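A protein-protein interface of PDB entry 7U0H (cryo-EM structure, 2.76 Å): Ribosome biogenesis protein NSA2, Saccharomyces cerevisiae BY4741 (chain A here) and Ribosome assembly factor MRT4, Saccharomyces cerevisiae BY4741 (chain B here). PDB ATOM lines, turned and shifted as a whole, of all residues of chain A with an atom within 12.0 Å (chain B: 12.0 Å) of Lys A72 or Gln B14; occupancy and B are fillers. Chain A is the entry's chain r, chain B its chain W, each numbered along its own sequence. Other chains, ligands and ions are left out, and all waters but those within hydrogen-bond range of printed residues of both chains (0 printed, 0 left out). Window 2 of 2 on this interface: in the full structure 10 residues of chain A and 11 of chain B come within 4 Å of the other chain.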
ATOM      1  N   LYS A  63       7.548 -29.634  -9.819  1.00  0.00           N
ATOM      2  CA  LYS A  63       6.981 -28.363  -9.377  1.00  0.00           C
ATOM      3  C   LYS A  63       8.067 -27.319  -9.180  1.00  0.00           C
ATOM      4  O   LYS A  63       7.888 -26.150  -9.537  1.00  0.00           O
ATOM      5  CB  LYS A  63       6.188 -28.549  -8.084  1.00  0.00           C
ATOM      6  CG  LYS A  63       4.788 -29.089  -8.280  1.00  0.00           C
ATOM      7  CD  LYS A  63       4.050 -29.192  -6.957  1.00  0.00           C
ATOM      8  CE  LYS A  63       2.655 -29.764  -7.151  1.00  0.00           C
ATOM      9  NZ  LYS A  63       1.862 -29.760  -5.887  1.00  0.00           N
ATOM     10  N   LYS A  64       9.202 -27.722  -8.607  1.00  0.00           N
ATOM     11  CA  LYS A  64      10.299 -26.790  -8.382  1.00  0.00           C
ATOM     12  C   LYS A  64      10.845 -26.242  -9.695  1.00  0.00           C
ATOM     13  O   LYS A  64      11.097 -25.037  -9.815  1.00  0.00           O
ATOM     14  CB  LYS A  64      11.404 -27.479  -7.585  1.00  0.00           C
ATOM     15  CG  LYS A  64      12.755 -26.823  -7.697  1.00  0.00           C
ATOM     16  CD  LYS A  64      13.852 -27.779  -7.268  1.00  0.00           C
ATOM     17  CE  LYS A  64      15.204 -27.092  -7.233  1.00  0.00           C
ATOM     18  NZ  LYS A  64      16.318 -28.059  -7.023  1.00  0.00           N
ATOM     19  N   ILE A  65      11.037 -27.107 -10.692  1.00  0.00           N
ATOM     20  CA  ILE A  65      11.553 -26.634 -11.975  1.00  0.00           C
ATOM     21  C   ILE A  65      10.557 -25.689 -12.634  1.00  0.00           C
ATOM     22  O   ILE A  65      10.937 -24.643 -13.182  1.00  0.00           O
ATOM     23  CB  ILE A  65      11.905 -27.821 -12.890  1.00  0.00           C
ATOM     24  CG1 ILE A  65      13.006 -28.669 -12.259  1.00  0.00           C
ATOM     25  CG2 ILE A  65      12.359 -27.329 -14.249  1.00  0.00           C
ATOM     26  CD1 ILE A  65      13.462 -29.819 -13.115  1.00  0.00           C
ATOM     27  N   LYS A  66       9.265 -26.034 -12.585  1.00  0.00           N
ATOM     28  CA  LYS A  66       8.254 -25.156 -13.166  1.00  0.00           C
ATOM     29  C   LYS A  66       8.242 -23.795 -12.479  1.00  0.00           C
ATOM     30  O   LYS A  66       8.162 -22.757 -13.145  1.00  0.00           O
ATOM     31  CB  LYS A  66       6.873 -25.804 -13.077  1.00  0.00           C
ATOM     32  CG  LYS A  66       6.713 -27.071 -13.899  1.00  0.00           C
ATOM     33  CD  LYS A  66       6.847 -26.797 -15.389  1.00  0.00           C
ATOM     34  CE  LYS A  66       5.813 -25.788 -15.861  1.00  0.00           C
ATOM     35  NZ  LYS A  66       5.639 -25.819 -17.339  1.00  0.00           N
ATOM     36  N   ALA A  67       8.323 -23.782 -11.148  1.00  0.00           N
ATOM     37  CA  ALA A  67       8.322 -22.523 -10.412  1.00  0.00           C
ATOM     38  C   ALA A  67       9.559 -21.696 -10.726  1.00  0.00           C
ATOM     39  O   ALA A  67       9.475 -20.470 -10.863  1.00  0.00           O
ATOM     40  CB  ALA A  67       8.227 -22.796  -8.913  1.00  0.00           C
ATOM     41  N   HIS A  68      10.721 -22.346 -10.829  1.00  0.00           N
ATOM     42  CA  HIS A  68      11.939 -21.624 -11.174  1.00  0.00           C
ATOM     43  C   HIS A  68      11.817 -20.980 -12.545  1.00  0.00           C
ATOM     44  O   HIS A  68      12.163 -19.807 -12.725  1.00  0.00           O
ATOM     45  CB  HIS A  68      13.138 -22.568 -11.132  1.00  0.00           C
ATOM     46  CG  HIS A  68      14.416 -21.942 -11.593  1.00  0.00           C
ATOM     47  ND1 HIS A  68      14.951 -22.170 -12.842  1.00  0.00           N
ATOM     48  CD2 HIS A  68      15.267 -21.093 -10.969  1.00  0.00           C
ATOM     49  CE1 HIS A  68      16.077 -21.491 -12.967  1.00  0.00           C
ATOM     50  NE2 HIS A  68      16.293 -20.832 -11.843  1.00  0.00           N
ATOM     51  N   GLU A  69      11.309 -21.729 -13.526  1.00  0.00           N
ATOM     52  CA  GLU A  69      11.161 -21.164 -14.862  1.00  0.00           C
ATOM     53  C   GLU A  69      10.134 -20.038 -14.884  1.00  0.00           C
ATOM     54  O   GLU A  69      10.329 -19.033 -15.574  1.00  0.00           O
ATOM     55  CB  GLU A  69      10.784 -22.254 -15.862  1.00  0.00           C
ATOM     56  CG  GLU A  69      11.982 -22.891 -16.537  1.00  0.00           C
ATOM     57  CD  GLU A  69      12.867 -21.871 -17.226  1.00  0.00           C
ATOM     58  OE1 GLU A  69      12.326 -20.960 -17.886  1.00  0.00           O
ATOM     59  OE2 GLU A  69      14.106 -21.974 -17.101  1.00  0.00           O
ATOM     60  N   GLN A  70       9.031 -20.184 -14.146  1.00  0.00           N
ATOM     61  CA  GLN A  70       8.002 -19.148 -14.147  1.00  0.00           C
ATOM     62  C   GLN A  70       8.500 -17.869 -13.486  1.00  0.00           C
ATOM     63  O   GLN A  70       8.239 -16.766 -13.981  1.00  0.00           O
ATOM     64  CB  GLN A  70       6.741 -19.660 -13.455  1.00  0.00           C
ATOM     65  CG  GLN A  70       5.531 -18.755 -13.617  1.00  0.00           C
ATOM     66  CD  GLN A  70       4.247 -19.395 -13.128  1.00  0.00           C
ATOM     67  OE1 GLN A  70       4.217 -20.583 -12.804  1.00  0.00           O
ATOM     68  NE2 GLN A  70       3.177 -18.611 -13.075  1.00  0.00           N
ATOM     69  N   SER A  71       9.218 -17.988 -12.364  1.00  0.00           N
ATOM     70  CA  SER A  71       9.804 -16.800 -11.750  1.00  0.00           C
ATOM     71  C   SER A  71      10.856 -16.180 -12.660  1.00  0.00           C
ATOM     72  O   SER A  71      10.943 -14.952 -12.774  1.00  0.00           O
ATOM     73  CB  SER A  71      10.407 -17.148 -10.387  1.00  0.00           C
ATOM     74  OG  SER A  71      11.628 -17.856 -10.526  1.00  0.00           O
ATOM     75  N   LYS A  72      11.659 -17.015 -13.324  1.00  0.00           N
ATOM     76  CA  LYS A  72      12.688 -16.515 -14.229  1.00  0.00           C
ATOM     77  C   LYS A  72      12.078 -15.745 -15.394  1.00  0.00           C
ATOM     78  O   LYS A  72      12.607 -14.707 -15.807  1.00  0.00           O
ATOM     79  CB  LYS A  72      13.522 -17.690 -14.730  1.00  0.00           C
ATOM     80  CG  LYS A  72      14.658 -17.338 -15.652  1.00  0.00           C
ATOM     81  CD  LYS A  72      15.326 -18.611 -16.138  1.00  0.00           C
ATOM     82  CE  LYS A  72      16.346 -18.322 -17.218  1.00  0.00           C
ATOM     83  NZ  LYS A  72      17.038 -19.559 -17.654  1.00  0.00           N
ATOM     84  N   VAL A  73      10.972 -16.248 -15.947  1.00  0.00           N
ATOM     85  CA  VAL A  73      10.258 -15.513 -16.988  1.00  0.00           C
ATOM     86  C   VAL A  73       9.688 -14.217 -16.425  1.00  0.00           C
ATOM     87  O   VAL A  73       9.792 -13.152 -17.047  1.00  0.00           O
ATOM     88  CB  VAL A  73       9.155 -16.395 -17.607  1.00  0.00           C
ATOM     89  CG1 VAL A  73       8.286 -15.581 -18.559  1.00  0.00           C
ATOM     90  CG2 VAL A  73       9.765 -17.590 -18.325  1.00  0.00           C
ATOM     91  N   LYS A  74       9.085 -14.286 -15.243  1.00  0.00           N
ATOM     92  CA  LYS A  74       8.495 -13.123 -14.588  1.00  0.00           C
ATOM     93  C   LYS A  74       9.525 -12.018 -14.362  1.00  0.00           C
ATOM     94  O   LYS A  74       9.418 -11.240 -13.416  1.00  0.00           O
ATOM     95  CB  LYS A  74       7.865 -13.533 -13.253  1.00  0.00           C
ATOM     96  CG  LYS A  74       6.548 -12.834 -12.945  1.00  0.00           C
ATOM     97  CD  LYS A  74       5.985 -13.249 -11.591  1.00  0.00           C
ATOM     98  CE  LYS A  74       5.513 -14.693 -11.592  1.00  0.00           C
ATOM     99  NZ  LYS A  74       4.663 -15.012 -10.405  1.00  0.00           N
ATOM    100  N   VAL B  10      20.806 -31.463 -13.770  1.00  0.00           N
ATOM    101  CA  VAL B  10      19.756 -30.454 -13.855  1.00  0.00           C
ATOM    102  C   VAL B  10      20.141 -29.316 -12.923  1.00  0.00           C
ATOM    103  O   VAL B  10      20.145 -29.477 -11.697  1.00  0.00           O
ATOM    104  CB  VAL B  10      18.381 -31.028 -13.493  1.00  0.00           C
ATOM    105  CG1 VAL B  10      17.314 -29.951 -13.598  1.00  0.00           C
ATOM    106  CG2 VAL B  10      18.050 -32.208 -14.390  1.00  0.00           C
ATOM    107  N   THR B  11      20.453 -28.159 -13.501  1.00  0.00           N
ATOM    108  CA  THR B  11      20.915 -27.007 -12.741  1.00  0.00           C
ATOM    109  C   THR B  11      20.053 -25.802 -13.078  1.00  0.00           C
ATOM    110  O   THR B  11      19.889 -25.460 -14.253  1.00  0.00           O
ATOM    111  CB  THR B  11      22.386 -26.709 -13.038  1.00  0.00           C
ATOM    112  OG1 THR B  11      22.554 -26.453 -14.439  1.00  0.00           O
ATOM    113  CG2 THR B  11      23.250 -27.882 -12.620  1.00  0.00           C
ATOM    114  N   LEU B  12      19.520 -25.156 -12.047  1.00  0.00           N
ATOM    115  CA  LEU B  12      18.620 -24.017 -12.206  1.00  0.00           C
ATOM    116  C   LEU B  12      19.446 -22.736 -12.120  1.00  0.00           C
ATOM    117  O   LEU B  12      19.609 -22.153 -11.051  1.00  0.00           O
ATOM    118  CB  LEU B  12      17.524 -24.045 -11.148  1.00  0.00           C
ATOM    119  CG  LEU B  12      16.646 -25.293 -11.092  1.00  0.00           C
ATOM    120  CD1 LEU B  12      15.468 -25.046 -10.172  1.00  0.00           C
ATOM    121  CD2 LEU B  12      16.170 -25.686 -12.480  1.00  0.00           C
ATOM    122  N   ALA B  13      19.961 -22.291 -13.263  1.00  0.00           N
ATOM    123  CA  ALA B  13      20.749 -21.072 -13.339  1.00  0.00           C
ATOM    124  C   ALA B  13      20.215 -20.180 -14.449  1.00  0.00           C
ATOM    125  O   ALA B  13      19.613 -20.656 -15.416  1.00  0.00           O
ATOM    126  CB  ALA B  13      22.230 -21.370 -13.568  1.00  0.00           C
ATOM    127  N   GLN B  14      20.447 -18.876 -14.297  1.00  0.00           N
ATOM    128  CA  GLN B  14      19.764 -17.888 -15.128  1.00  0.00           C
ATOM    129  C   GLN B  14      20.236 -17.932 -16.578  1.00  0.00           C
ATOM    130  O   GLN B  14      19.418 -17.974 -17.502  1.00  0.00           O
ATOM    131  CB  GLN B  14      19.966 -16.493 -14.535  1.00  0.00           C
ATOM    132  CG  GLN B  14      19.546 -16.383 -13.077  1.00  0.00           C
ATOM    133  CD  GLN B  14      18.060 -16.601 -12.877  1.00  0.00           C
ATOM    134  OE1 GLN B  14      17.286 -16.596 -13.833  1.00  0.00           O
ATOM    135  NE2 GLN B  14      17.653 -16.792 -11.630  1.00  0.00           N
ATOM    136  N   THR B  15      21.547 -17.922 -16.800  1.00  0.00           N
ATOM    137  CA  THR B  15      22.062 -17.742 -18.151  1.00  0.00           C
ATOM    138  C   THR B  15      21.764 -18.965 -19.010  1.00  0.00           C
ATOM    139  O   THR B  15      22.033 -20.101 -18.611  1.00  0.00           O
ATOM    140  CB  THR B  15      23.563 -17.473 -18.115  1.00  0.00           C
ATOM    141  OG1 THR B  15      23.846 -16.487 -17.117  1.00  0.00           O
ATOM    142  CG2 THR B  15      24.035 -16.958 -19.456  1.00  0.00           C
ATOM    143  N   ASP B  16      21.209 -18.726 -20.196  1.00  0.00           N
ATOM    144  CA  ASP B  16      20.865 -19.778 -21.140  1.00  0.00           C
ATOM    145  C   ASP B  16      21.711 -19.646 -22.397  1.00  0.00           C
ATOM    146  O   ASP B  16      22.014 -18.534 -22.838  1.00  0.00           O
ATOM    147  CB  ASP B  16      19.382 -19.725 -21.509  1.00  0.00           C
ATOM    148  CG  ASP B  16      19.043 -20.633 -22.671  1.00  0.00           C
ATOM    149  OD1 ASP B  16      19.073 -21.870 -22.489  1.00  0.00           O
ATOM    150  OD2 ASP B  16      18.751 -20.114 -23.771  1.00  0.00           O
ATOM    151  N   LYS B  17      22.093 -20.785 -22.971  1.00  0.00           N
ATOM    152  CA  LYS B  17      22.882 -20.775 -24.194  1.00  0.00           C
ATOM    153  C   LYS B  17      22.111 -20.089 -25.315  1.00  0.00           C
ATOM    154  O   LYS B  17      20.943 -20.398 -25.567  1.00  0.00           O
ATOM    155  CB  LYS B  17      23.265 -22.201 -24.583  1.00  0.00           C
ATOM    156  CG  LYS B  17      22.135 -23.205 -24.523  1.00  0.00           C
ATOM    157  CD  LYS B  17      22.693 -24.613 -24.402  1.00  0.00           C
ATOM    158  CE  LYS B  17      21.654 -25.664 -24.753  1.00  0.00           C
ATOM    159  NZ  LYS B  17      21.404 -25.748 -26.219  1.00  0.00           N
ATOM    160  N   LYS B  18      22.775 -19.148 -25.987  1.00  0.00           N
ATOM    161  CA  LYS B  18      22.055 -18.203 -26.835  1.00  0.00           C
ATOM    162  C   LYS B  18      21.584 -18.852 -28.133  1.00  0.00           C
ATOM    163  O   LYS B  18      20.448 -18.628 -28.566  1.00  0.00           O
ATOM    164  CB  LYS B  18      22.931 -16.983 -27.121  1.00  0.00           C
ATOM    165  CG  LYS B  18      22.879 -15.901 -26.042  1.00  0.00           C
ATOM    166  CD  LYS B  18      23.531 -16.344 -24.739  1.00  0.00           C
ATOM    167  CE  LYS B  18      24.994 -16.681 -24.957  1.00  0.00           C
ATOM    168  NZ  LYS B  18      25.672 -17.101 -23.700  1.00  0.00           N
ATOM    169  N   GLY B  19      22.434 -19.653 -28.766  1.00  0.00           N
ATOM    170  CA  GLY B  19      22.033 -20.347 -29.973  1.00  0.00           C
ATOM    171  C   GLY B  19      22.445 -19.670 -31.264  1.00  0.00           C
ATOM    172  O   GLY B  19      23.459 -18.969 -31.315  1.00  0.00           O
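Lys A72 touches two residues of chain B. Gln B14 touches one residue of chain A. His A68 touches just these residues of chain B: Leu B12 and Ala B13. No residue of chain B comes within 4 Å of Ser A71. No residue of chain B comes within 4 Å of Val A73. Of the printed residues of chain A, Ala B13 touches His A68 (3.98 Å) and Lys A72 (3.6 Å). Asp B16 touches none of the printed residues of chain A. Of the printed residues of chain A, Leu B12 touches Lys A64 (3.6 Å) and His A68 (3.5 Å). Of the printed residues of chain B, Lys A64 touches Leu B12. Of the printed residues of chain B, Ile A65 touches Val B10 (3.9 Å). Printed residues of chain A within 4 Å of Val B10: Ile A65 (3.9 Å). The nearest residue of chain A that does not touch Gln B14 is His A68 (4.3 Å).
CD1 of Leu B12 touches CE of Lys A64, at 3.6 Å. Ile A65 touches Val B10 (CD1 to CG1, 3.9 Å). Leu B12 touches His A68 (CB to CE1, 3.5 Å). His A68 touches Ala B13. Ala B13 touches Lys A72.
The side-chain carboxylate (OE2) of Glu A69 is in salt-bridge range of the side-chain amino group (NZ) of Lys A72 (3.8 Å). The backbone carbonyl oxygen of His A68 lies within hydrogen-bond range of the side-chain hydroxyl of Ser A71, at 3.0 Å.
Of the 10 printed residues of chain B, 4 touch a printed residue of chain A. Along chain B the printed residues that touch a printed residue of chain A span positions 10 to 14. Hydrophobic or aromatic side chains of chain A that line the printed part of chain B: Ile A65 and His A68. Among the printed residues, no Asp or Glu carboxylate lies within 4 Å of a Lys or Arg side-chain nitrogen of the other chain.
The backbone carbonyl oxygen of Gln B14 is in hydrogen-bond range of the side-chain amino group of Lys A72, 2.9 Å away.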
